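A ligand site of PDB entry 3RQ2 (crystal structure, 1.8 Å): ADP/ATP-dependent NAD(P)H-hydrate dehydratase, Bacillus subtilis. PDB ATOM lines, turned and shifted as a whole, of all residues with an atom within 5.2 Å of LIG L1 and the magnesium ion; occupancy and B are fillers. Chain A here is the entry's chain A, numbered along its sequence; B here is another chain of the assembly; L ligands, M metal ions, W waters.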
ATOM      1  N   ASP A 131      -4.140  -0.453 -19.445  1.00  0.00           N
ATOM      2  CA  ASP A 131      -4.697   0.810 -18.965  1.00  0.00           C
ATOM      3  C   ASP A 131      -5.592   0.579 -17.762  1.00  0.00           C
ATOM      4  O   ASP A 131      -6.098  -0.526 -17.531  1.00  0.00           O
ATOM      5  CB  ASP A 131      -5.548   1.445 -20.111  1.00  0.00           C
ATOM      6  CG  ASP A 131      -6.010   2.873 -19.803  1.00  0.00           C
ATOM      7  OD1 ASP A 131      -5.350   3.553 -18.976  1.00  0.00           O
ATOM      8  OD2 ASP A 131      -7.097   3.255 -20.319  1.00  0.00           O
ATOM      9  N   ALA A 132      -5.853   1.653 -17.019  1.00  0.00           N
ATOM     10  CA  ALA A 132      -6.943   1.670 -16.069  1.00  0.00           C
ATOM     11  C   ALA A 132      -6.965   0.458 -15.105  1.00  0.00           C
ATOM     12  O   ALA A 132      -5.995   0.285 -14.310  1.00  0.00           O
ATOM     13  CB  ALA A 132      -8.282   1.796 -16.811  1.00  0.00           C
ATOM     14  N   HIS A 152      -2.515   7.656 -15.916  1.00  0.00           N
ATOM     15  CA  HIS A 152      -2.503   9.019 -15.385  1.00  0.00           C
ATOM     16  C   HIS A 152      -1.732   9.027 -14.064  1.00  0.00           C
ATOM     17  O   HIS A 152      -1.347   7.983 -13.565  1.00  0.00           O
ATOM     18  CB  HIS A 152      -3.901   9.596 -15.266  1.00  0.00           C
ATOM     19  CG  HIS A 152      -4.820   8.856 -14.352  1.00  0.00           C
ATOM     20  ND1 HIS A 152      -4.484   8.464 -13.064  1.00  0.00           N
ATOM     21  CD2 HIS A 152      -6.121   8.494 -14.535  1.00  0.00           C
ATOM     22  CE1 HIS A 152      -5.532   7.881 -12.502  1.00  0.00           C
ATOM     23  NE2 HIS A 152      -6.531   7.869 -13.377  1.00  0.00           N
ATOM     24  N   GLU A 155      -2.681   6.500 -11.356  1.00  0.00           N
ATOM     25  CA  GLU A 155      -2.376   5.120 -11.675  1.00  0.00           C
ATOM     26  C   GLU A 155      -0.866   4.876 -11.548  1.00  0.00           C
ATOM     27  O   GLU A 155      -0.426   3.788 -11.121  1.00  0.00           O
ATOM     28  CB  GLU A 155      -2.893   4.808 -13.069  1.00  0.00           C
ATOM     29  CG  GLU A 155      -4.414   4.664 -13.084  1.00  0.00           C
ATOM     30  CD  GLU A 155      -5.112   4.889 -14.378  1.00  0.00           C
ATOM     31  OE1 GLU A 155      -4.544   5.454 -15.341  1.00  0.00           O
ATOM     32  OE2 GLU A 155      -6.321   4.536 -14.428  1.00  0.00           O
ATOM     33  N   LYS A 189       0.195  10.321 -18.567  1.00  0.00           N
ATOM     34  CA  LYS A 189      -0.771  11.299 -19.057  1.00  0.00           C
ATOM     35  C   LYS A 189      -0.781  12.569 -18.196  1.00  0.00           C
ATOM     36  O   LYS A 189      -0.199  12.614 -17.083  1.00  0.00           O
ATOM     37  CB  LYS A 189      -2.125  10.604 -19.125  1.00  0.00           C
ATOM     38  CG  LYS A 189      -2.102   9.597 -20.294  1.00  0.00           C
ATOM     39  CD  LYS A 189      -2.780   8.274 -20.065  1.00  0.00           C
ATOM     40  CE  LYS A 189      -4.250   8.385 -19.923  1.00  0.00           C
ATOM     41  NZ  LYS A 189      -4.888   7.116 -19.502  1.00  0.00           N
ATOM     42  N   GLY A 190      -1.437  13.590 -18.758  1.00  0.00           N
ATOM     43  CA  GLY A 190      -1.519  14.905 -18.180  1.00  0.00           C
ATOM     44  C   GLY A 190      -1.188  15.938 -19.265  1.00  0.00           C
ATOM     45  O   GLY A 190      -0.842  15.586 -20.420  1.00  0.00           O
ATOM     46  N   ASN A 191      -1.318  17.213 -18.916  1.00  0.00           N
ATOM     47  CA  ASN A 191      -0.754  18.258 -19.735  1.00  0.00           C
ATOM     48  C   ASN A 191       0.721  17.868 -19.983  1.00  0.00           C
ATOM     49  O   ASN A 191       1.397  17.375 -19.069  1.00  0.00           O
ATOM     50  CB  ASN A 191      -0.858  19.595 -18.989  1.00  0.00           C
ATOM     51  CG  ASN A 191      -0.215  20.741 -19.732  1.00  0.00           C
ATOM     52  OD1 ASN A 191      -0.421  20.942 -20.920  1.00  0.00           O
ATOM     53  ND2 ASN A 191       0.561  21.533 -18.996  1.00  0.00           N
ATOM     54  N   THR A 193       1.873  15.262 -21.807  1.00  0.00           N
ATOM     55  CA  THR A 193       2.023  13.813 -21.646  1.00  0.00           C
ATOM     56  C   THR A 193       3.471  13.376 -22.013  1.00  0.00           C
ATOM     57  O   THR A 193       4.044  13.852 -23.009  1.00  0.00           O
ATOM     58  CB  THR A 193       1.014  13.076 -22.496  1.00  0.00           C
ATOM     59  OG1 THR A 193      -0.314  13.206 -21.906  1.00  0.00           O
ATOM     60  CG2 THR A 193       1.397  11.556 -22.648  1.00  0.00           C
ATOM     61  N   THR A 207       0.315  18.621 -27.762  1.00  0.00           N
ATOM     62  CA  THR A 207      -1.087  18.945 -28.121  1.00  0.00           C
ATOM     63  C   THR A 207      -2.054  18.598 -26.955  1.00  0.00           C
ATOM     64  O   THR A 207      -1.730  17.831 -26.031  1.00  0.00           O
ATOM     65  CB  THR A 207      -1.540  18.140 -29.351  1.00  0.00           C
ATOM     66  OG1 THR A 207      -1.514  16.746 -29.010  1.00  0.00           O
ATOM     67  CG2 THR A 207      -0.658  18.371 -30.543  1.00  0.00           C
ATOM     68  N   GLY A 208      -3.279  19.127 -27.037  1.00  0.00           N
ATOM     69  CA  GLY A 208      -4.271  18.870 -25.993  1.00  0.00           C
ATOM     70  C   GLY A 208      -4.488  20.105 -25.125  1.00  0.00           C
ATOM     71  O   GLY A 208      -3.683  21.088 -25.105  1.00  0.00           O
ATOM     72  N   ASN A 209      -5.626  20.101 -24.468  1.00  0.00           N
ATOM     73  CA  ASN A 209      -6.012  21.144 -23.559  1.00  0.00           C
ATOM     74  C   ASN A 209      -7.044  20.652 -22.547  1.00  0.00           C
ATOM     75  O   ASN A 209      -7.333  19.411 -22.457  1.00  0.00           O
ATOM     76  CB  ASN A 209      -6.514  22.373 -24.365  1.00  0.00           C
ATOM     77  CG  ASN A 209      -7.717  22.060 -25.249  1.00  0.00           C
ATOM     78  OD1 ASN A 209      -8.607  21.292 -24.838  1.00  0.00           O
ATOM     79  ND2 ASN A 209      -7.768  22.660 -26.459  1.00  0.00           N
ATOM     80  N   GLY A 210      -7.551  21.600 -21.748  1.00  0.00           N
ATOM     81  CA  GLY A 210      -8.477  21.273 -20.680  1.00  0.00           C
ATOM     82  C   GLY A 210      -9.823  20.670 -21.104  1.00  0.00           C
ATOM     83  O   GLY A 210     -10.532  20.096 -20.283  1.00  0.00           O
ATOM     84  N   LEU A 212      -9.981  17.995 -22.527  1.00  0.00           N
ATOM     85  CA  LEU A 212      -9.710  16.565 -22.222  1.00  0.00           C
ATOM     86  C   LEU A 212      -9.870  16.170 -20.770  1.00  0.00           C
ATOM     87  O   LEU A 212      -9.872  14.982 -20.437  1.00  0.00           O
ATOM     88  CB  LEU A 212      -8.294  16.187 -22.740  1.00  0.00           C
ATOM     89  CG  LEU A 212      -8.032  16.328 -24.250  1.00  0.00           C
ATOM     90  CD1 LEU A 212      -6.539  16.084 -24.554  1.00  0.00           C
ATOM     91  CD2 LEU A 212      -8.969  15.368 -25.074  1.00  0.00           C
ATOM     92  N   ALA A 213      -9.986  17.151 -19.886  1.00  0.00           N
ATOM     93  CA  ALA A 213     -10.043  16.947 -18.434  1.00  0.00           C
ATOM     94  C   ALA A 213     -11.484  16.543 -18.016  1.00  0.00           C
ATOM     95  O   ALA A 213     -12.179  17.256 -17.286  1.00  0.00           O
ATOM     96  CB  ALA A 213      -9.600  18.216 -17.691  1.00  0.00           C
ATOM     97  N   LYS A 214     -11.878  15.379 -18.491  1.00  0.00           N
ATOM     98  CA  LYS A 214     -13.245  14.875 -18.289  1.00  0.00           C
ATOM     99  C   LYS A 214     -13.272  13.402 -18.564  1.00  0.00           C
ATOM    100  O   LYS A 214     -12.556  12.900 -19.437  1.00  0.00           O
ATOM    101  CB  LYS A 214     -14.262  15.569 -19.216  1.00  0.00           C
ATOM    102  CG  LYS A 214     -15.734  15.324 -18.821  1.00  0.00           C
ATOM    103  CD  LYS A 214     -16.749  16.052 -19.698  1.00  0.00           C
ATOM    104  CE  LYS A 214     -16.633  17.588 -19.670  1.00  0.00           C
ATOM    105  NZ  LYS A 214     -17.489  18.227 -20.757  1.00  0.00           N
ATOM    106  N   GLY A 216     -13.536   9.687 -19.567  1.00  0.00           N
ATOM    107  CA  GLY A 216     -13.612   8.941 -20.795  1.00  0.00           C
ATOM    108  C   GLY A 216     -12.547   9.242 -21.810  1.00  0.00           C
ATOM    109  O   GLY A 216     -12.308   8.448 -22.727  1.00  0.00           O
ATOM    110  N   THR A 217     -11.899  10.379 -21.703  1.00  0.00           N
ATOM    111  CA  THR A 217     -10.934  10.719 -22.713  1.00  0.00           C
ATOM    112  C   THR A 217      -9.722   9.786 -22.747  1.00  0.00           C
ATOM    113  O   THR A 217      -9.166   9.543 -23.838  1.00  0.00           O
ATOM    114  CB  THR A 217     -10.491  12.165 -22.592  1.00  0.00           C
ATOM    115  OG1 THR A 217      -9.895  12.362 -21.289  1.00  0.00           O
ATOM    116  CG2 THR A 217     -11.661  13.105 -22.784  1.00  0.00           C
ATOM    117  N   GLY A 218      -9.299   9.287 -21.604  1.00  0.00           N
ATOM    118  CA  GLY A 218      -8.238   8.289 -21.588  1.00  0.00           C
ATOM    119  C   GLY A 218      -8.662   6.927 -22.146  1.00  0.00           C
ATOM    120  O   GLY A 218      -7.826   6.184 -22.682  1.00  0.00           O
ATOM    121  N   ASP A 219      -9.967   6.578 -21.999  1.00  0.00           N
ATOM    122  CA  ASP A 219     -10.511   5.361 -22.571  1.00  0.00           C
ATOM    123  C   ASP A 219     -10.460   5.419 -24.091  1.00  0.00           C
ATOM    124  O   ASP A 219     -10.005   4.491 -24.761  1.00  0.00           O
ATOM    125  CB  ASP A 219     -11.935   5.091 -22.024  1.00  0.00           C
ATOM    126  CG  ASP A 219     -11.955   5.081 -20.511  1.00  0.00           C
ATOM    127  OD1 ASP A 219     -11.032   4.492 -19.866  1.00  0.00           O
ATOM    128  OD2 ASP A 219     -12.900   5.696 -19.959  1.00  0.00           O
ATOM    129  N   LEU A 221      -8.331   7.312 -25.777  1.00  0.00           N
ATOM    130  CA  LEU A 221      -6.900   7.263 -26.122  1.00  0.00           C
ATOM    131  C   LEU A 221      -6.390   5.816 -26.233  1.00  0.00           C
ATOM    132  O   LEU A 221      -5.677   5.448 -27.169  1.00  0.00           O
ATOM    133  CB  LEU A 221      -6.051   8.049 -25.119  1.00  0.00           C
ATOM    134  CG  LEU A 221      -4.526   7.952 -25.377  1.00  0.00           C
ATOM    135  CD1 LEU A 221      -4.107   8.533 -26.739  1.00  0.00           C
ATOM    136  CD2 LEU A 221      -3.712   8.611 -24.209  1.00  0.00           C
ATOM    137  N   HIS A 246      -4.835  12.555 -30.596  1.00  0.00           N
ATOM    138  CA  HIS A 246      -5.797  12.665 -29.519  1.00  0.00           C
ATOM    139  C   HIS A 246      -5.897  14.101 -28.997  1.00  0.00           C
ATOM    140  O   HIS A 246      -6.983  14.651 -28.922  1.00  0.00           O
ATOM    141  CB  HIS A 246      -5.437  11.639 -28.421  1.00  0.00           C
ATOM    142  CG  HIS A 246      -6.290  11.651 -27.192  1.00  0.00           C
ATOM    143  ND1 HIS A 246      -5.864  12.285 -26.040  1.00  0.00           N
ATOM    144  CD2 HIS A 246      -7.471  11.036 -26.890  1.00  0.00           C
ATOM    145  CE1 HIS A 246      -6.773  12.064 -25.085  1.00  0.00           C
ATOM    146  NE2 HIS A 246      -7.759  11.341 -25.591  1.00  0.00           N
ATOM    147  N   ASP B  22      -8.235  25.385 -17.047  1.00  0.00           N
ATOM    148  CA  ASP B  22      -6.783  25.562 -17.219  1.00  0.00           C
ATOM    149  C   ASP B  22      -6.089  24.381 -17.876  1.00  0.00           C
ATOM    150  O   ASP B  22      -6.477  23.214 -17.656  1.00  0.00           O
ATOM    151  CB  ASP B  22      -6.036  25.864 -15.907  1.00  0.00           C
ATOM    152  CG  ASP B  22      -4.681  26.523 -16.164  1.00  0.00           C
ATOM    153  OD1 ASP B  22      -4.687  27.653 -16.732  1.00  0.00           O
ATOM    154  OD2 ASP B  22      -3.594  25.925 -15.851  1.00  0.00           O
ATOM    155  N   ALA B  23      -5.032  24.726 -18.612  1.00  0.00           N
ATOM    156  CA  ALA B  23      -4.083  23.801 -19.208  1.00  0.00           C
ATOM    157  C   ALA B  23      -3.587  22.794 -18.177  1.00  0.00           C
ATOM    158  O   ALA B  23      -3.479  21.624 -18.495  1.00  0.00           O
ATOM    159  CB  ALA B  23      -2.915  24.544 -19.807  1.00  0.00           C
ATOM    160  N   GLU B  24      -3.337  23.252 -16.947  1.00  0.00           N
ATOM    161  CA  GLU B  24      -2.840  22.369 -15.884  1.00  0.00           C
ATOM    162  C   GLU B  24      -3.973  21.849 -14.980  1.00  0.00           C
ATOM    163  O   GLU B  24      -4.047  22.238 -13.797  1.00  0.00           O
ATOM    164  CB  GLU B  24      -1.859  23.151 -14.983  1.00  0.00           C
ATOM    165  CG  GLU B  24      -0.745  23.844 -15.718  1.00  0.00           C
ATOM    166  CD  GLU B  24       0.448  24.119 -14.820  1.00  0.00           C
ATOM    167  OE1 GLU B  24       0.276  24.820 -13.785  1.00  0.00           O
ATOM    168  OE2 GLU B  24       1.572  23.658 -15.132  1.00  0.00           O
ATOM    169  N   SER B  25      -4.913  21.104 -15.550  1.00  0.00           N
ATOM    170  CA  SER B  25      -6.047  20.543 -14.816  1.00  0.00           C
ATOM    171  C   SER B  25      -6.299  19.147 -15.335  1.00  0.00           C
ATOM    172  O   SER B  25      -5.853  18.802 -16.429  1.00  0.00           O
ATOM    173  CB  SER B  25      -7.306  21.411 -14.993  1.00  0.00           C
ATOM    174  OG  SER B  25      -7.741  21.479 -16.343  1.00  0.00           O
ATOM    175  N   HIS B  26      -6.984  18.338 -14.548  1.00  0.00           N
ATOM    176  CA  HIS B  26      -7.457  17.036 -14.969  1.00  0.00           C
ATOM    177  C   HIS B  26      -8.883  16.854 -14.552  1.00  0.00           C
ATOM    178  O   HIS B  26      -9.452  17.742 -13.907  1.00  0.00           O
ATOM    179  CB  HIS B  26      -6.568  15.909 -14.405  1.00  0.00           C
ATOM    180  CG  HIS B  26      -6.561  15.835 -12.915  1.00  0.00           C
ATOM    181  ND1 HIS B  26      -7.261  14.862 -12.209  1.00  0.00           N
ATOM    182  CD2 HIS B  26      -5.937  16.602 -11.983  1.00  0.00           C
ATOM    183  CE1 HIS B  26      -7.061  15.048 -10.922  1.00  0.00           C
ATOM    184  NE2 HIS B  26      -6.274  16.101 -10.756  1.00  0.00           N
ATOM    185  N   LYS B  27      -9.505  15.730 -14.903  1.00  0.00           N
ATOM    186  CA  LYS B  27     -10.926  15.582 -14.597  1.00  0.00           C
ATOM    187  C   LYS B  27     -11.214  15.792 -13.088  1.00  0.00           C
ATOM    188  O   LYS B  27     -12.270  16.321 -12.716  1.00  0.00           O
ATOM    189  CB  LYS B  27     -11.457  14.211 -15.077  1.00  0.00           C
ATOM    190  CG  LYS B  27     -10.796  12.998 -14.459  1.00  0.00           C
ATOM    191  CD  LYS B  27     -11.305  11.721 -15.194  1.00  0.00           C
ATOM    192  CE  LYS B  27     -10.845  10.431 -14.462  1.00  0.00           C
ATOM    193  NZ  LYS B  27      -9.355  10.273 -14.477  1.00  0.00           N
HETATM  194  P1  LIG L   1      -7.786   9.523 -18.164  1.00  0.00           P
HETATM  195  O1  LIG L   1      -9.245   9.602 -18.650  1.00  0.00           O
HETATM  196  O2  LIG L   1      -7.677  10.248 -16.877  1.00  0.00           O
HETATM  197  O3  LIG L   1      -7.299   8.117 -18.208  1.00  0.00           O
HETATM  198  O4  LIG L   1      -6.992  10.242 -19.282  1.00  0.00           O
HETATM  199  C1  LIG L   1      -7.136  11.635 -19.464  1.00  0.00           C
HETATM  200  C2  LIG L   1      -6.638  12.023 -20.846  1.00  0.00           C
HETATM  201  O5  LIG L   1      -6.877  13.412 -21.102  1.00  0.00           O
HETATM  202  C3  LIG L   1      -5.146  11.890 -21.044  1.00  0.00           C
HETATM  203  O6  LIG L   1      -4.815  11.600 -22.411  1.00  0.00           O
HETATM  204  C4  LIG L   1      -4.605  13.240 -20.610  1.00  0.00           C
HETATM  205  O7  LIG L   1      -3.245  13.472 -21.025  1.00  0.00           O
HETATM  206  C5  LIG L   1      -5.640  14.155 -21.226  1.00  0.00           C
HETATM  207  N1  LIG L   1      -5.800  15.392 -20.490  1.00  0.00           N
HETATM  208  C6  LIG L   1      -6.566  15.650 -19.392  1.00  0.00           C
HETATM  209  N2  LIG L   1      -6.489  16.961 -19.013  1.00  0.00           N
HETATM  210  C7  LIG L   1      -5.665  17.554 -19.895  1.00  0.00           C
HETATM  211  C8  LIG L   1      -5.138  18.918 -20.089  1.00  0.00           C
HETATM  212  N3  LIG L   1      -5.525  19.818 -19.186  1.00  0.00           N
HETATM  213  N4  LIG L   1      -4.307  19.136 -21.142  1.00  0.00           N
HETATM  214  C9  LIG L   1      -3.965  18.168 -22.001  1.00  0.00           C
HETATM  215  N5  LIG L   1      -4.409  16.880 -21.875  1.00  0.00           N
HETATM  216  C10 LIG L   1      -5.240  16.556 -20.882  1.00  0.00           C
HETATM  217  P1  LG2 L   2      -9.127   6.761 -10.375  1.00  0.00           P
HETATM  218  O1  LG2 L   2      -9.671   6.941  -8.984  1.00  0.00           O
HETATM  219  O2  LG2 L   2      -8.439   5.496 -10.681  1.00  0.00           O
HETATM  220  O3  LG2 L   2      -8.061   7.921 -10.698  1.00  0.00           O
HETATM  221  C1  LG2 L   2      -8.326   9.339 -10.540  1.00  0.00           C
HETATM  222  C2  LG2 L   2      -7.341   9.904  -9.514  1.00  0.00           C
HETATM  223  O4  LG2 L   2      -6.009   9.861 -10.030  1.00  0.00           O
HETATM  224  C3  LG2 L   2      -7.593  11.356  -9.154  1.00  0.00           C
HETATM  225  O5  LG2 L   2      -8.546  11.425  -8.095  1.00  0.00           O
HETATM  226  C4  LG2 L   2      -6.220  11.856  -8.773  1.00  0.00           C
HETATM  227  O6  LG2 L   2      -5.902  11.356  -7.483  1.00  0.00           O
HETATM  228  C5  LG2 L   2      -5.356  11.111  -9.756  1.00  0.00           C
HETATM  229  N1  LG2 L   2      -5.093  11.801 -11.022  1.00  0.00           N
HETATM  230  C6  LG2 L   2      -5.496  11.457 -12.274  1.00  0.00           C
HETATM  231  N2  LG2 L   2      -5.031  12.321 -13.186  1.00  0.00           N
HETATM  232  C7  LG2 L   2      -4.260  13.239 -12.508  1.00  0.00           C
HETATM  233  C8  LG2 L   2      -3.437  14.416 -12.894  1.00  0.00           C
HETATM  234  N3  LG2 L   2      -3.303  14.838 -14.156  1.00  0.00           N
HETATM  235  N4  LG2 L   2      -2.831  15.077 -11.885  1.00  0.00           N
HETATM  236  C9  LG2 L   2      -2.939  14.682 -10.588  1.00  0.00           C
HETATM  237  N5  LG2 L   2      -3.647  13.611 -10.137  1.00  0.00           N
HETATM  238  C10 LG2 L   2      -4.320  12.883 -11.094  1.00  0.00           C
HETATM  239  O7  LG2 L   2     -10.390   7.029 -11.348  1.00  0.00           O
HETATM  240  P2  LG2 L   2     -10.434   6.913 -12.966  1.00  0.00           P
HETATM  241  O8  LG2 L   2      -9.311   7.585 -13.709  1.00  0.00           O
HETATM  242  O9  LG2 L   2     -11.832   7.448 -13.255  1.00  0.00           O
HETATM  243  O10 LG2 L   2     -10.345   5.343 -13.415  1.00  0.00           O
HETATM  244  C11 LG2 L   2     -11.172   4.408 -12.682  1.00  0.00           C
HETATM  245  C12 LG2 L   2     -11.891   3.532 -13.711  1.00  0.00           C
HETATM  246  O11 LG2 L   2     -13.028   4.284 -14.248  1.00  0.00           O
HETATM  247  C13 LG2 L   2     -11.075   3.001 -14.886  1.00  0.00           C
HETATM  248  O12 LG2 L   2     -11.336   1.589 -15.193  1.00  0.00           O
HETATM  249  C14 LG2 L   2     -11.508   3.878 -16.035  1.00  0.00           C
HETATM  250  O13 LG2 L   2     -11.314   3.277 -17.355  1.00  0.00           O
HETATM  251  C15 LG2 L   2     -13.001   3.999 -15.653  1.00  0.00           C
HETATM  252  N6  LG2 L   2     -13.715   5.053 -16.362  1.00  0.00           N
HETATM  253  C16 LG2 L   2     -14.789   4.726 -17.000  1.00  0.00           C
HETATM  254  C17 LG2 L   2     -15.615   5.587 -17.570  1.00  0.00           C
HETATM  255  C18 LG2 L   2     -16.780   5.100 -18.355  1.00  0.00           C
HETATM  256  O14 LG2 L   2     -17.081   3.884 -18.437  1.00  0.00           O
HETATM  257  N7  LG2 L   2     -17.483   6.044 -19.017  1.00  0.00           N
HETATM  258  C19 LG2 L   2     -15.297   7.117 -17.519  1.00  0.00           C
HETATM  259  C20 LG2 L   2     -14.426   7.416 -16.312  1.00  0.00           C
HETATM  260  C21 LG2 L   2     -13.227   6.418 -16.299  1.00  0.00           C
HETATM  261  O15 LG2 L   2     -12.475   6.615 -17.499  1.00  0.00           O
HETATM  262 MG    MG M   1      -7.958   6.351 -17.583  1.00  0.00          MG
HETATM  263  O   HOH W   1      -6.488  12.304 -15.713  1.00  0.00           O
HETATM  264  O   HOH W   2     -11.804   9.270 -17.453  1.00  0.00           O
HETATM  265  O   HOH W   3      -2.840  21.268 -21.777  1.00  0.00           O
HETATM  266  O   HOH W   4      -2.890  14.948 -23.342  1.00  0.00           O
HETATM  267  O   HOH W   5      -8.244   5.883 -15.606  1.00  0.00           O
HETATM  268  O   HOH W   6      -8.278  14.046 -16.838  1.00  0.00           O
HETATM  269  O   HOH W   7      -2.281  11.739 -23.404  1.00  0.00           O
HETATM  270  O   HOH W   8      -9.894   7.278 -17.745  1.00  0.00           O
HETATM  271  O   HOH W   9      -8.393   5.117 -19.169  1.00  0.00           O
HETATM  272  O   HOH W  10     -10.151  12.181 -18.112  1.00  0.00           O
HETATM  273  O   HOH W  11      -4.226  16.603 -17.000  1.00  0.00           O
HETATM  274  O   HOH W  12      -6.053   5.582 -17.519  1.00  0.00           O
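N4 of LIG L1 lies close to O of Asn 209, 3.3 Å away. The backbone carbonyl oxygen of Leu 212 lies close to an oxygen (O5) of LIG L1, at 3.4 Å. His 152 touches LIG L1. CA of Asn 191 touches N4 of LIG L1, 3.9 Å away. C of Gly 208 touches C9 of LIG L1 (3.7 Å). CA of Gly 210 touches N3 of LIG L1 (3.6 Å). Ala 213 touches LIG L1 (CA to N2, 3.6 Å). CD2 of Leu 221 touches O6 of LIG L1 (3.7 Å). CE1 of His 246 touches O6 of LIG L1 (3.3 Å). Asp 22 of chain B touches LIG L1 (O to N3, 3.8 Å). Hydrophobic or aromatic side chains that line LIG L1: His 152, Leu 212, Ala 213, Leu 221 and His 246.
OG1 of Thr 193 is in hydrogen-bond range of O of Gly 190, at 2.9 Å. NZ of Lys 189 is in salt-bridge range of OD1 of Asp 131, at 3.6 Å. The backbone carbonyl oxygen of Asp 22 of chain B lies within hydrogen-bond range of the side-chain hydroxyl of Ser 25 of chain B, at 2.5 Å. O of Thr 217 sits at hydrogen-bond distance from NE2 of His 246, at 2.9 Å. OG1 of Thr 217 is in hydrogen-bond range of O of Leu 212 (2.8 Å). The backbone carbonyl oxygen (O) of Lys 214 sits at hydrogen-bond distance from the side-chain hydroxyl (OG1) of Thr 217. The backbone NH (N) of His 152 sits at hydrogen-bond distance from the side-chain carboxylate (OE1) of Glu 155 (3.0 Å). The backbone NH (N) of Glu 24 of chain B is in hydrogen-bond range of the side-chain carboxylate (OD2) of Asp 22 of chain B (2.9 Å).
Residues that only touch the magnesium ion: Glu 155 and Lys 189. Of the 27 residues printed, 2 come within 4 Å of the magnesium ion.
Water W12 lies within hydrogen-bond range of the side-chain carboxylate of Asp 131 (2.6 Å), the side-chain carboxylate of Glu 155 (2.7 Å) and the side-chain amino group of Lys 189 (2.8 Å). Water W9 lies within hydrogen-bond range of the side-chain carboxylate of Asp 131 (2.5 Å) and the side-chain carboxylate of Asp 219 (2.8 Å). Water W5 lies within hydrogen-bond range of the side-chain carboxylate (OE2) of Glu 155, an oxygen (O8) of LG2 L2 and a ring nitrogen (NE2) of His 152. Water W4 bridges an oxygen (O7) of LIG L1 (2.8 Å) and the side-chain hydroxyl of Thr 193 (3.4 Å). Water W2 lies within hydrogen-bond range of an oxygen (O15) of LG2 L2, the backbone NH of Gly 216 and an oxygen (O1) of LIG L1. Water W11 lies within hydrogen-bond range of O of Ser 25 of chain B (2.8 Å), N2 of LIG L1 (3.0 Å) and N3 of LG2 L2 (3.5 Å).
The magnesium ion is bound by O3 of LIG L1 (2.0 Å), water W5 (2.1 Å), water W12 (2.1 Å), water W9 (2.1 Å) and water W8 (2.2 Å). The magnesium ion has five donor atoms within binding distance.
The backbone carbonyl oxygen (O) of Ala 23 of chain B is in hydrogen-bond range of a nitrogen (N3) of LIG L1. The backbone NH of Gly 190 is in hydrogen-bond range of an oxygen (O7) of LIG L1, 2.9 Å away. O of Gly 190 is in hydrogen-bond range of O7 of LIG L1 (3.3 Å). An oxygen (O3) of LIG L1 sits close to the side-chain amino group (NZ) of Lys 189 (2.9 Å). The side-chain amino group of Lys 27 of chain B is in salt-bridge range of an oxygen (O2) of LIG L1, at 2.9 Å. The backbone carbonyl oxygen (O) of Ser 25 of chain B sits at hydrogen-bond distance from a nitrogen (N3) of LIG L1 (3.0 Å). N of Gly 218 sits at hydrogen-bond distance from O1 of LIG L1 (3.0 Å). An oxygen (O7) of LIG L1 sits at hydrogen-bond distance from the side-chain hydroxyl of Thr 193. The side-chain hydroxyl of Thr 217 lies within hydrogen-bond range of an oxygen (O5) of LIG L1, 3.2 Å away. NZ of Lys 27 of chain B lies within salt-bridge range of O8 of LG2 L2. A ring nitrogen (NE2) of His 152 lies within hydrogen-bond range of an oxygen (O8) of LG2 L2 (2.8 Å). OD2 of Asp 219 is in hydrogen-bond range of O15 of LG2 L2, at 2.7 Å.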
